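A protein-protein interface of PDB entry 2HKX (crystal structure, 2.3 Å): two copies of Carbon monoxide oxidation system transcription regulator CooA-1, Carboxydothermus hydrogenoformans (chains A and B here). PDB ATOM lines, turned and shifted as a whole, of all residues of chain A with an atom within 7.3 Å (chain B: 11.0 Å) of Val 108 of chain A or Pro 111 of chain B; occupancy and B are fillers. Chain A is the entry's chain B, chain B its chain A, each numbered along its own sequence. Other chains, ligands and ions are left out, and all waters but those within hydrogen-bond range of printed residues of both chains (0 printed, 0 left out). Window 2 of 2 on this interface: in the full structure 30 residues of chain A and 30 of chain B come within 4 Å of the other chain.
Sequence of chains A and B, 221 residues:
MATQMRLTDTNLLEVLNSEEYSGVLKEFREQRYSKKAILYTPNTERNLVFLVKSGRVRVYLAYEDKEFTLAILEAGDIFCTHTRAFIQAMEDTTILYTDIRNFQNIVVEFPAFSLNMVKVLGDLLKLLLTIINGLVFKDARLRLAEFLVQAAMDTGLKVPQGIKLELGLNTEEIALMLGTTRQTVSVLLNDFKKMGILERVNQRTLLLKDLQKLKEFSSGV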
ATOM      1  N   ASN A 102      14.600 -23.281  25.541  1.00  0.00           N
ATOM      2  CA  ASN A 102      15.527 -22.648  26.473  1.00  0.00           C
ATOM      3  C   ASN A 102      16.192 -21.414  25.880  1.00  0.00           C
ATOM      4  O   ASN A 102      16.264 -20.380  26.540  1.00  0.00           O
ATOM      5  CB  ASN A 102      16.646 -23.603  26.857  1.00  0.00           C
ATOM      6  CG  ASN A 102      16.206 -24.698  27.788  1.00  0.00           C
ATOM      7  OD1 ASN A 102      16.953 -25.649  27.999  1.00  0.00           O
ATOM      8  ND2 ASN A 102      15.003 -24.584  28.358  1.00  0.00           N
ATOM      9  N   PHE A 103      16.682 -21.540  24.645  1.00  0.00           N
ATOM     10  CA  PHE A 103      17.309 -20.418  23.928  1.00  0.00           C
ATOM     11  C   PHE A 103      16.377 -19.218  23.828  1.00  0.00           C
ATOM     12  O   PHE A 103      16.811 -18.087  24.034  1.00  0.00           O
ATOM     13  CB  PHE A 103      17.815 -20.843  22.536  1.00  0.00           C
ATOM     14  CG  PHE A 103      18.550 -19.758  21.795  1.00  0.00           C
ATOM     15  CD1 PHE A 103      19.850 -19.379  22.179  1.00  0.00           C
ATOM     16  CD2 PHE A 103      17.960 -19.123  20.705  1.00  0.00           C
ATOM     17  CE1 PHE A 103      20.535 -18.376  21.487  1.00  0.00           C
ATOM     18  CE2 PHE A 103      18.625 -18.131  20.023  1.00  0.00           C
ATOM     19  CZ  PHE A 103      19.920 -17.757  20.406  1.00  0.00           C
ATOM     20  N   GLN A 104      15.099 -19.463  23.552  1.00  0.00           N
ATOM     21  CA  GLN A 104      14.096 -18.383  23.576  1.00  0.00           C
ATOM     22  C   GLN A 104      13.859 -17.761  24.968  1.00  0.00           C
ATOM     23  O   GLN A 104      13.697 -16.543  25.082  1.00  0.00           O
ATOM     24  CB  GLN A 104      12.794 -18.826  22.895  1.00  0.00           C
ATOM     25  CG  GLN A 104      12.975 -18.987  21.368  1.00  0.00           C
ATOM     26  CD  GLN A 104      11.779 -19.602  20.636  1.00  0.00           C
ATOM     27  OE1 GLN A 104      10.794 -20.045  21.255  1.00  0.00           O
ATOM     28  NE2 GLN A 104      11.865 -19.637  19.299  1.00  0.00           N
ATOM     29  N   ASN A 105      13.848 -18.585  26.017  1.00  0.00           N
ATOM     30  CA  ASN A 105      13.782 -18.083  27.399  1.00  0.00           C
ATOM     31  C   ASN A 105      15.015 -17.227  27.757  1.00  0.00           C
ATOM     32  O   ASN A 105      14.900 -16.202  28.422  1.00  0.00           O
ATOM     33  CB  ASN A 105      13.660 -19.239  28.403  1.00  0.00           C
ATOM     34  CG  ASN A 105      12.272 -19.902  28.422  1.00  0.00           C
ATOM     35  OD1 ASN A 105      11.255 -19.311  28.033  1.00  0.00           O
ATOM     36  ND2 ASN A 105      12.236 -21.147  28.899  1.00  0.00           N
ATOM     37  N   ILE A 106      16.192 -17.668  27.322  1.00  0.00           N
ATOM     38  CA  ILE A 106      17.431 -16.907  27.465  1.00  0.00           C
ATOM     39  C   ILE A 106      17.320 -15.539  26.770  1.00  0.00           C
ATOM     40  O   ILE A 106      17.565 -14.489  27.385  1.00  0.00           O
ATOM     41  CB  ILE A 106      18.639 -17.701  26.877  1.00  0.00           C
ATOM     42  CG1 ILE A 106      18.935 -18.947  27.744  1.00  0.00           C
ATOM     43  CG2 ILE A 106      19.881 -16.782  26.694  1.00  0.00           C
ATOM     44  CD1 ILE A 106      19.804 -19.985  27.068  1.00  0.00           C
ATOM     45  N   VAL A 107      16.954 -15.570  25.487  1.00  0.00           N
ATOM     46  CA  VAL A 107      16.833 -14.367  24.667  1.00  0.00           C
ATOM     47  C   VAL A 107      15.847 -13.366  25.282  1.00  0.00           C
ATOM     48  O   VAL A 107      16.023 -12.172  25.143  1.00  0.00           O
ATOM     49  CB  VAL A 107      16.464 -14.733  23.188  1.00  0.00           C
ATOM     50  CG1 VAL A 107      15.969 -13.546  22.434  1.00  0.00           C
ATOM     51  CG2 VAL A 107      17.675 -15.351  22.471  1.00  0.00           C
ATOM     52  N   VAL A 108      14.829 -13.868  25.975  1.00  0.00           N
ATOM     53  CA  VAL A 108      13.825 -13.031  26.634  1.00  0.00           C
ATOM     54  C   VAL A 108      14.292 -12.552  28.015  1.00  0.00           C
ATOM     55  O   VAL A 108      14.021 -11.419  28.392  1.00  0.00           O
ATOM     56  CB  VAL A 108      12.451 -13.762  26.729  1.00  0.00           C
ATOM     57  CG1 VAL A 108      11.596 -13.247  27.911  1.00  0.00           C
ATOM     58  CG2 VAL A 108      11.706 -13.647  25.411  1.00  0.00           C
ATOM     59  N   GLU A 109      14.998 -13.401  28.756  1.00  0.00           N
ATOM     60  CA  GLU A 109      15.538 -12.996  30.060  1.00  0.00           C
ATOM     61  C   GLU A 109      16.684 -12.003  29.935  1.00  0.00           C
ATOM     62  O   GLU A 109      16.852 -11.148  30.809  1.00  0.00           O
ATOM     63  CB  GLU A 109      16.002 -14.205  30.895  1.00  0.00           C
ATOM     64  CG  GLU A 109      15.438 -14.161  32.315  1.00  0.00           C
ATOM     65  CD  GLU A 109      16.437 -14.522  33.413  1.00  0.00           C
ATOM     66  OE1 GLU A 109      17.176 -15.519  33.249  1.00  0.00           O
ATOM     67  OE2 GLU A 109      16.456 -13.817  34.453  1.00  0.00           O
ATOM     68  N   PHE A 110      17.449 -12.133  28.843  1.00  0.00           N
ATOM     69  CA  PHE A 110      18.669 -11.379  28.559  1.00  0.00           C
ATOM     70  C   PHE A 110      18.619 -10.845  27.113  1.00  0.00           C
ATOM     71  O   PHE A 110      19.318 -11.350  26.245  1.00  0.00           O
ATOM     72  CB  PHE A 110      19.900 -12.293  28.726  1.00  0.00           C
ATOM     73  CG  PHE A 110      20.180 -12.697  30.170  1.00  0.00           C
ATOM     74  CD1 PHE A 110      20.974 -11.895  30.993  1.00  0.00           C
ATOM     75  CD2 PHE A 110      19.642 -13.866  30.698  1.00  0.00           C
ATOM     76  CE1 PHE A 110      21.224 -12.246  32.331  1.00  0.00           C
ATOM     77  CE2 PHE A 110      19.877 -14.228  32.050  1.00  0.00           C
ATOM     78  CZ  PHE A 110      20.676 -13.417  32.858  1.00  0.00           C
ATOM     79  N   PRO A 111      17.807  -9.799  26.854  1.00  0.00           N
ATOM     80  CA  PRO A 111      17.534  -9.443  25.462  1.00  0.00           C
ATOM     81  C   PRO A 111      18.770  -8.968  24.708  1.00  0.00           C
ATOM     82  O   PRO A 111      18.785  -9.042  23.489  1.00  0.00           O
ATOM     83  CB  PRO A 111      16.522  -8.300  25.582  1.00  0.00           C
ATOM     84  CG  PRO A 111      15.998  -8.373  26.995  1.00  0.00           C
ATOM     85  CD  PRO A 111      17.145  -8.878  27.789  1.00  0.00           C
ATOM     86  N   ALA A 112      19.796  -8.505  25.435  1.00  0.00           N
ATOM     87  CA  ALA A 112      21.011  -7.958  24.811  1.00  0.00           C
ATOM     88  C   ALA A 112      21.889  -9.053  24.260  1.00  0.00           C
ATOM     89  O   ALA A 112      22.721  -8.805  23.398  1.00  0.00           O
ATOM     90  CB  ALA A 112      21.797  -7.093  25.793  1.00  0.00           C
ATOM     91  N   SER A 114      20.903 -11.295  22.286  1.00  0.00           N
ATOM     92  CA  SER A 114      20.530 -11.287  20.880  1.00  0.00           C
ATOM     93  C   SER A 114      21.357 -10.367  20.013  1.00  0.00           C
ATOM     94  O   SER A 114      21.514 -10.629  18.822  1.00  0.00           O
ATOM     95  CB  SER A 114      19.078 -10.838  20.743  1.00  0.00           C
ATOM     96  OG  SER A 114      18.221 -11.887  21.124  1.00  0.00           O
ATOM     97  N   THR B  10       4.490 -14.032  11.663  1.00  0.00           N
ATOM     98  CA  THR B  10       4.731 -13.332  12.939  1.00  0.00           C
ATOM     99  C   THR B  10       4.167 -11.904  12.976  1.00  0.00           C
ATOM    100  O   THR B  10       4.292 -11.158  12.002  1.00  0.00           O
ATOM    101  CB  THR B  10       6.236 -13.318  13.309  1.00  0.00           C
ATOM    102  OG1 THR B  10       6.855 -14.543  12.886  1.00  0.00           O
ATOM    103  CG2 THR B  10       6.415 -13.164  14.822  1.00  0.00           C
ATOM    104  N   LEU B  12       4.435  -8.489  14.357  1.00  0.00           N
ATOM    105  CA  LEU B  12       5.247  -7.434  14.963  1.00  0.00           C
ATOM    106  C   LEU B  12       4.538  -6.075  14.966  1.00  0.00           C
ATOM    107  O   LEU B  12       5.103  -5.080  15.419  1.00  0.00           O
ATOM    108  CB  LEU B  12       6.580  -7.320  14.216  1.00  0.00           C
ATOM    109  CG  LEU B  12       7.920  -7.120  14.938  1.00  0.00           C
ATOM    110  CD1 LEU B  12       8.978  -6.767  13.902  1.00  0.00           C
ATOM    111  CD2 LEU B  12       7.893  -6.076  16.047  1.00  0.00           C
ATOM    112  N   VAL B  15       2.165  -5.802  18.419  1.00  0.00           N
ATOM    113  CA  VAL B  15       3.092  -5.525  19.506  1.00  0.00           C
ATOM    114  C   VAL B  15       3.353  -4.020  19.609  1.00  0.00           C
ATOM    115  O   VAL B  15       3.115  -3.410  20.657  1.00  0.00           O
ATOM    116  CB  VAL B  15       4.422  -6.299  19.309  1.00  0.00           C
ATOM    117  CG1 VAL B  15       5.420  -5.953  20.396  1.00  0.00           C
ATOM    118  CG2 VAL B  15       4.165  -7.801  19.289  1.00  0.00           C
ATOM    119  N   GLU B  20       1.927  -1.997  26.441  1.00  0.00           N
ATOM    120  CA  GLU B  20       3.182  -1.417  26.928  1.00  0.00           C
ATOM    121  C   GLU B  20       3.814  -0.478  25.905  1.00  0.00           C
ATOM    122  O   GLU B  20       4.346   0.580  26.258  1.00  0.00           O
ATOM    123  CB  GLU B  20       4.185  -2.521  27.299  1.00  0.00           C
ATOM    124  CG  GLU B  20       3.623  -3.651  28.162  1.00  0.00           C
ATOM    125  CD  GLU B  20       3.104  -4.823  27.330  1.00  0.00           C
ATOM    126  OE1 GLU B  20       3.800  -5.926  27.381  1.00  0.00           O
ATOM    127  OE2 GLU B  20       2.008  -4.648  26.621  1.00  0.00           O
ATOM    128  N   TYR B  21       3.730  -0.875  24.635  1.00  0.00           N
ATOM    129  CA  TYR B  21       4.454  -0.221  23.553  1.00  0.00           C
ATOM    130  C   TYR B  21       3.725   1.021  23.039  1.00  0.00           C
ATOM    131  O   TYR B  21       2.658   0.889  22.305  1.00  0.00           O
ATOM    132  CB  TYR B  21       4.697  -1.215  22.410  1.00  0.00           C
ATOM    133  CG  TYR B  21       5.368  -2.519  22.819  1.00  0.00           C
ATOM    134  CD1 TYR B  21       4.677  -3.492  23.549  1.00  0.00           C
ATOM    135  CD2 TYR B  21       6.685  -2.783  22.459  1.00  0.00           C
ATOM    136  CE1 TYR B  21       5.288  -4.686  23.925  1.00  0.00           C
ATOM    137  CE2 TYR B  21       7.305  -3.986  22.815  1.00  0.00           C
ATOM    138  CZ  TYR B  21       6.605  -4.930  23.552  1.00  0.00           C
ATOM    139  OH  TYR B  21       7.219  -6.112  23.910  1.00  0.00           O
ATOM    140  N   VAL B  24       8.262   3.514  22.327  1.00  0.00           N
ATOM    141  CA  VAL B  24       9.257   3.002  21.367  1.00  0.00           C
ATOM    142  C   VAL B  24       8.931   3.425  19.890  1.00  0.00           C
ATOM    143  O   VAL B  24       9.855   3.729  19.010  1.00  0.00           O
ATOM    144  CB  VAL B  24       9.410   1.427  21.481  1.00  0.00           C
ATOM    145  CG1 VAL B  24       8.053   0.724  21.457  1.00  0.00           C
ATOM    146  CG2 VAL B  24      10.313   0.859  20.386  1.00  0.00           C
ATOM    147  N   PHE B 103      18.024   1.002  17.704  1.00  0.00           N
ATOM    148  CA  PHE B 103      17.372  -0.320  17.768  1.00  0.00           C
ATOM    149  C   PHE B 103      17.970  -1.232  18.829  1.00  0.00           C
ATOM    150  O   PHE B 103      17.263  -1.980  19.500  1.00  0.00           O
ATOM    151  CB  PHE B 103      17.416  -1.032  16.429  1.00  0.00           C
ATOM    152  CG  PHE B 103      16.518  -2.219  16.372  1.00  0.00           C
ATOM    153  CD1 PHE B 103      15.137  -2.055  16.328  1.00  0.00           C
ATOM    154  CD2 PHE B 103      17.039  -3.501  16.387  1.00  0.00           C
ATOM    155  CE1 PHE B 103      14.289  -3.141  16.297  1.00  0.00           C
ATOM    156  CE2 PHE B 103      16.197  -4.602  16.344  1.00  0.00           C
ATOM    157  CZ  PHE B 103      14.820  -4.420  16.293  1.00  0.00           C
ATOM    158  N   GLN B 104      19.282  -1.148  18.977  1.00  0.00           N
ATOM    159  CA  GLN B 104      19.992  -1.919  19.981  1.00  0.00           C
ATOM    160  C   GLN B 104      19.553  -1.556  21.403  1.00  0.00           C
ATOM    161  O   GLN B 104      19.566  -2.398  22.297  1.00  0.00           O
ATOM    162  CB  GLN B 104      21.495  -1.765  19.765  1.00  0.00           C
ATOM    163  CG  GLN B 104      21.923  -2.331  18.404  1.00  0.00           C
ATOM    164  CD  GLN B 104      23.346  -1.988  18.031  1.00  0.00           C
ATOM    165  OE1 GLN B 104      23.901  -0.966  18.466  1.00  0.00           O
ATOM    166  NE2 GLN B 104      23.956  -2.846  17.221  1.00  0.00           N
ATOM    167  N   ASN B 105      19.141  -0.304  21.587  1.00  0.00           N
ATOM    168  CA  ASN B 105      18.577   0.169  22.853  1.00  0.00           C
ATOM    169  C   ASN B 105      17.139  -0.312  23.091  1.00  0.00           C
ATOM    170  O   ASN B 105      16.782  -0.695  24.198  1.00  0.00           O
ATOM    171  CB  ASN B 105      18.650   1.700  22.925  1.00  0.00           C
ATOM    172  CG  ASN B 105      20.079   2.223  23.048  1.00  0.00           C
ATOM    173  OD1 ASN B 105      21.052   1.497  22.820  1.00  0.00           O
ATOM    174  ND2 ASN B 105      20.208   3.492  23.415  1.00  0.00           N
ATOM    175  N   ILE B 106      16.328  -0.287  22.037  1.00  0.00           N
ATOM    176  CA  ILE B 106      14.930  -0.744  22.065  1.00  0.00           C
ATOM    177  C   ILE B 106      14.753  -2.236  22.412  1.00  0.00           C
ATOM    178  O   ILE B 106      13.757  -2.635  23.031  1.00  0.00           O
ATOM    179  CB  ILE B 106      14.260  -0.501  20.693  1.00  0.00           C
ATOM    180  CG1 ILE B 106      14.015   0.995  20.462  1.00  0.00           C
ATOM    181  CG2 ILE B 106      12.974  -1.321  20.565  1.00  0.00           C
ATOM    182  CD1 ILE B 106      14.200   1.437  19.028  1.00  0.00           C
ATOM    183  N   VAL B 107      15.709  -3.055  21.996  1.00  0.00           N
ATOM    184  CA  VAL B 107      15.594  -4.503  22.183  1.00  0.00           C
ATOM    185  C   VAL B 107      15.614  -4.903  23.683  1.00  0.00           C
ATOM    186  O   VAL B 107      14.928  -5.846  24.100  1.00  0.00           O
ATOM    187  CB  VAL B 107      16.623  -5.268  21.283  1.00  0.00           C
ATOM    188  CG1 VAL B 107      16.641  -6.739  21.576  1.00  0.00           C
ATOM    189  CG2 VAL B 107      16.295  -5.054  19.812  1.00  0.00           C
ATOM    190  N   VAL B 108      16.350  -4.149  24.495  1.00  0.00           N
ATOM    191  CA  VAL B 108      16.528  -4.496  25.906  1.00  0.00           C
ATOM    192  C   VAL B 108      15.408  -3.923  26.800  1.00  0.00           C
ATOM    193  O   VAL B 108      15.135  -4.445  27.885  1.00  0.00           O
ATOM    194  CB  VAL B 108      17.953  -4.126  26.401  1.00  0.00           C
ATOM    195  CG1 VAL B 108      18.973  -4.363  25.279  1.00  0.00           C
ATOM    196  CG2 VAL B 108      18.020  -2.683  26.870  1.00  0.00           C
ATOM    197  N   GLU B 109      14.759  -2.864  26.321  1.00  0.00           N
ATOM    198  CA  GLU B 109      13.616  -2.271  27.009  1.00  0.00           C
ATOM    199  C   GLU B 109      12.362  -3.113  26.771  1.00  0.00           C
ATOM    200  O   GLU B 109      11.410  -3.073  27.559  1.00  0.00           O
ATOM    201  CB  GLU B 109      13.401  -0.821  26.536  1.00  0.00           C
ATOM    202  CG  GLU B 109      13.329   0.197  27.670  1.00  0.00           C
ATOM    203  CD  GLU B 109      14.499   0.079  28.640  1.00  0.00           C
ATOM    204  OE1 GLU B 109      15.661   0.010  28.176  1.00  0.00           O
ATOM    205  OE2 GLU B 109      14.250   0.045  29.867  1.00  0.00           O
ATOM    206  N   PHE B 110      12.378  -3.873  25.671  1.00  0.00           N
ATOM    207  CA  PHE B 110      11.268  -4.735  25.280  1.00  0.00           C
ATOM    208  C   PHE B 110      11.785  -6.048  24.694  1.00  0.00           C
ATOM    209  O   PHE B 110      12.122  -6.112  23.499  1.00  0.00           O
ATOM    210  CB  PHE B 110      10.376  -4.029  24.261  1.00  0.00           C
ATOM    211  CG  PHE B 110       9.904  -2.660  24.702  1.00  0.00           C
ATOM    212  CD1 PHE B 110       8.860  -2.527  25.613  1.00  0.00           C
ATOM    213  CD2 PHE B 110      10.501  -1.508  24.194  1.00  0.00           C
ATOM    214  CE1 PHE B 110       8.426  -1.270  26.020  1.00  0.00           C
ATOM    215  CE2 PHE B 110      10.071  -0.248  24.584  1.00  0.00           C
ATOM    216  CZ  PHE B 110       9.032  -0.127  25.503  1.00  0.00           C
ATOM    217  N   PRO B 111      11.828  -7.108  25.521  1.00  0.00           N
ATOM    218  CA  PRO B 111      12.365  -8.418  25.127  1.00  0.00           C
ATOM    219  C   PRO B 111      11.639  -9.064  23.935  1.00  0.00           C
ATOM    220  O   PRO B 111      12.212  -9.935  23.264  1.00  0.00           O
ATOM    221  CB  PRO B 111      12.167  -9.270  26.383  1.00  0.00           C
ATOM    222  CG  PRO B 111      12.047  -8.271  27.515  1.00  0.00           C
ATOM    223  CD  PRO B 111      11.347  -7.103  26.916  1.00  0.00           C
ATOM    224  N   ALA B 112      10.401  -8.638  23.677  1.00  0.00           N
ATOM    225  CA  ALA B 112       9.596  -9.197  22.594  1.00  0.00           C
ATOM    226  C   ALA B 112      10.186  -8.905  21.214  1.00  0.00           C
ATOM    227  O   ALA B 112       9.993  -9.679  20.277  1.00  0.00           O
ATOM    228  CB  ALA B 112       8.189  -8.694  22.675  1.00  0.00           C
ATOM    229  N   PHE B 113      10.880  -7.778  21.095  1.00  0.00           N
ATOM    230  CA  PHE B 113      11.620  -7.438  19.884  1.00  0.00           C
ATOM    231  C   PHE B 113      12.795  -8.384  19.719  1.00  0.00           C
ATOM    232  O   PHE B 113      12.969  -8.994  18.658  1.00  0.00           O
ATOM    233  CB  PHE B 113      12.129  -6.000  19.948  1.00  0.00           C
ATOM    234  CG  PHE B 113      11.152  -4.990  19.443  1.00  0.00           C
ATOM    235  CD1 PHE B 113      10.246  -4.391  20.309  1.00  0.00           C
ATOM    236  CD2 PHE B 113      11.134  -4.640  18.094  1.00  0.00           C
ATOM    237  CE1 PHE B 113       9.332  -3.453  19.847  1.00  0.00           C
ATOM    238  CE2 PHE B 113      10.228  -3.703  17.616  1.00  0.00           C
ATOM    239  CZ  PHE B 113       9.324  -3.108  18.490  1.00  0.00           C
ATOM    240  N   SER B 114      13.584  -8.524  20.784  1.00  0.00           N
ATOM    241  CA  SER B 114      14.707  -9.445  20.802  1.00  0.00           C
ATOM    242  C   SER B 114      14.294 -10.814  20.284  1.00  0.00           C
ATOM    243  O   SER B 114      14.884 -11.311  19.323  1.00  0.00           O
ATOM    244  CB  SER B 114      15.295  -9.551  22.206  1.00  0.00           C
ATOM    245  OG  SER B 114      16.411 -10.425  22.209  1.00  0.00           O
ATOM    246  N   LEU B 115      13.255 -11.377  20.905  1.00  0.00           N
ATOM    247  CA  LEU B 115      12.699 -12.687  20.590  1.00  0.00           C
ATOM    248  C   LEU B 115      12.158 -12.791  19.151  1.00  0.00           C
ATOM    249  O   LEU B 115      12.232 -13.856  18.518  1.00  0.00           O
ATOM    250  CB  LEU B 115      11.604 -13.003  21.610  1.00  0.00           C
ATOM    251  CG  LEU B 115      10.656 -14.192  21.424  1.00  0.00           C
ATOM    252  CD1 LEU B 115      11.355 -15.520  21.677  1.00  0.00           C
ATOM    253  CD2 LEU B 115       9.455 -14.042  22.348  1.00  0.00           C
ATOM    254  N   ASN B 116      11.609 -11.683  18.654  1.00  0.00           N
ATOM    255  CA  ASN B 116      11.150 -11.588  17.274  1.00  0.00           C
ATOM    256  C   ASN B 116      12.329 -11.551  16.314  1.00  0.00           C
ATOM    257  O   ASN B 116      12.349 -12.245  15.299  1.00  0.00           O
ATOM    258  CB  ASN B 116      10.272 -10.344  17.083  1.00  0.00           C
ATOM    259  CG  ASN B 116       9.800 -10.169  15.645  1.00  0.00           C
ATOM    260  OD1 ASN B 116      10.418  -9.449  14.861  1.00  0.00           O
ATOM    261  ND2 ASN B 116       8.700 -10.832  15.291  1.00  0.00           N
ATOM    262  N   MET B 117      13.325 -10.740  16.638  1.00  0.00           N
ATOM    263  CA  MET B 117      14.449 -10.582  15.747  1.00  0.00           C
ATOM    264  C   MET B 117      15.226 -11.901  15.617  1.00  0.00           C
ATOM    265  O   MET B 117      15.764 -12.177  14.551  1.00  0.00           O
ATOM    266  CB  MET B 117      15.317  -9.360  16.117  1.00  0.00           C
ATOM    267  CG  MET B 117      16.543  -9.638  16.940  1.00  0.00           C
ATOM    268  SD  MET B 117      17.803  -8.340  16.804  1.00  0.00           S
ATOM    269  CE  MET B 117      17.711  -8.052  15.027  1.00  0.00           C
ATOM    270  N   VAL B 118      15.214 -12.744  16.657  1.00  0.00           N
ATOM    271  CA  VAL B 118      15.865 -14.068  16.566  1.00  0.00           C
ATOM    272  C   VAL B 118      15.099 -15.089  15.732  1.00  0.00           C
ATOM    273  O   VAL B 118      15.724 -15.919  15.043  1.00  0.00           O
ATOM    274  CB  VAL B 118      16.311 -14.692  17.944  1.00  0.00           C
ATOM    275  CG1 VAL B 118      15.675 -14.028  19.114  1.00  0.00           C
ATOM    276  CG2 VAL B 118      16.051 -16.212  17.996  1.00  0.00           C
ATOM    277  N   LYS B 119      13.767 -15.034  15.810  1.00  0.00           N
ATOM    278  CA  LYS B 119      12.873 -15.929  15.075  1.00  0.00           C
ATOM    279  C   LYS B 119      12.914 -15.618  13.568  1.00  0.00           C
ATOM    280  O   LYS B 119      12.893 -16.512  12.734  1.00  0.00           O
ATOM    281  CB  LYS B 119      11.452 -15.820  15.656  1.00  0.00           C
ATOM    282  CG  LYS B 119      10.310 -16.465  14.861  1.00  0.00           C
ATOM    283  CD  LYS B 119      10.426 -17.987  14.714  1.00  0.00           C
ATOM    284  CE  LYS B 119       9.266 -18.534  13.877  1.00  0.00           C
ATOM    285  NZ  LYS B 119       9.279 -20.026  13.729  1.00  0.00           N
ATOM    286  N   VAL B 120      12.994 -14.334  13.249  1.00  0.00           N
ATOM    287  CA  VAL B 120      13.106 -13.843  11.890  1.00  0.00           C
ATOM    288  C   VAL B 120      14.473 -14.206  11.281  1.00  0.00           C
ATOM    289  O   VAL B 120      14.540 -14.715  10.160  1.00  0.00           O
ATOM    290  CB  VAL B 120      12.805 -12.312  11.853  1.00  0.00           C
ATOM    291  CG1 VAL B 120      13.370 -11.618  10.597  1.00  0.00           C
ATOM    292  CG2 VAL B 120      11.283 -12.074  12.013  1.00  0.00           C
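Of the printed residues of chain B, Phe 103 of chain A touches Val 118.
Of chain B, only Ser 114, Leu 115 and Val 118 come within 4 Å of Val 107 of chain A.
No residue of chain B comes within 4 Å of Glu 109 of chain A.
Printed residues of chain B within 4 Å of Ser 114 of chain A: Ser 114 (2.6 Å) and Val 118 (3.9 Å).
Of the printed residues of chain A, Val 108 of chain B touches Pro 111 (3.8 Å) and Ala 112 (3.96 Å).
Printed residues of chain A within 4 Å of Pro 111 of chain B: Val 108 (3.5 Å) and Pro 111 (3.98 Å).
The nearest printed residue of chain A that does not touch Pro 111 of chain B is Val 107 of chain A (4.8 Å).
The side-chain hydroxyl (OG) of Ser 114 of chain B sits close to the backbone carbonyl oxygen (O) of Val 107 of chain A (3.4 Å).
O of Pro 111 of chain A is in hydrogen-bond range of OG of Ser 114 of chain B (3.0 Å).
OG of Ser 114 of chain B sits at hydrogen-bond distance from OG of Ser 114 of chain A (2.6 Å).
Among the printed residues, merely in contact across the chains: Phe 103 of chain A with Val 118 of chain B (3.8 Å), Gln 104 of chain A with Leu 115 of chain B (3.8 Å), Val 107 of chain A with Leu 115 of chain B (3.8 Å), Val 107 of chain A with Val 118 of chain B (3.4 Å), Val 108 of chain A with Pro 111 of chain B (3.5 Å), Val 108 of chain A with Leu 115 of chain B (3.8 Å), Pro 111 of chain A with Val 107 of chain B (3.3 Å), Pro 111 of chain A with Val 108 of chain B (3.8 Å), Pro 111 of chain A with Pro 111 of chain B (3.98 Å), Ala 112 of chain A with Val 108 of chain B (3.96 Å) and Ser 114 of chain A with Val 118 of chain B (3.9 Å).
Printed residues of chain B that touch a printed residue of chain A: Val 107, Val 108, Pro 111, Ser 114, Leu 115 and Val 118.
Hydrophobic or aromatic side chains of chain B within 4 Å of the printed part of chain A: Val 107, Val 108, Pro 111, Leu 115 and Val 118.
Hydrophobic or aromatic side chains of chain A within 4 Å of the printed part of chain B: Phe 103, Val 107, Val 108, Pro 111 and Ala 112.
Among the printed residues, 14 pairs touch across the chains.
Val 108 of chain A touches Pro 111 of chain B, and with the chains exchanged Pro 111 of chain A touches Val 108 of chain B.
Pro 111 of chain A touches Val 107 of chain B, but with the chains exchanged Val 107 of chain A does not touch Pro 111 of chain B (4.8 Å).
Ala 112 of chain A touches Val 108 of chain B, but with the chains exchanged Val 108 of chain A does not touch Ala 112 of chain B (5.5 Å).
Ser 114 of chain B touches its own counterpart, Ser 114 of chain A.
11 positions are printed for both chains.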
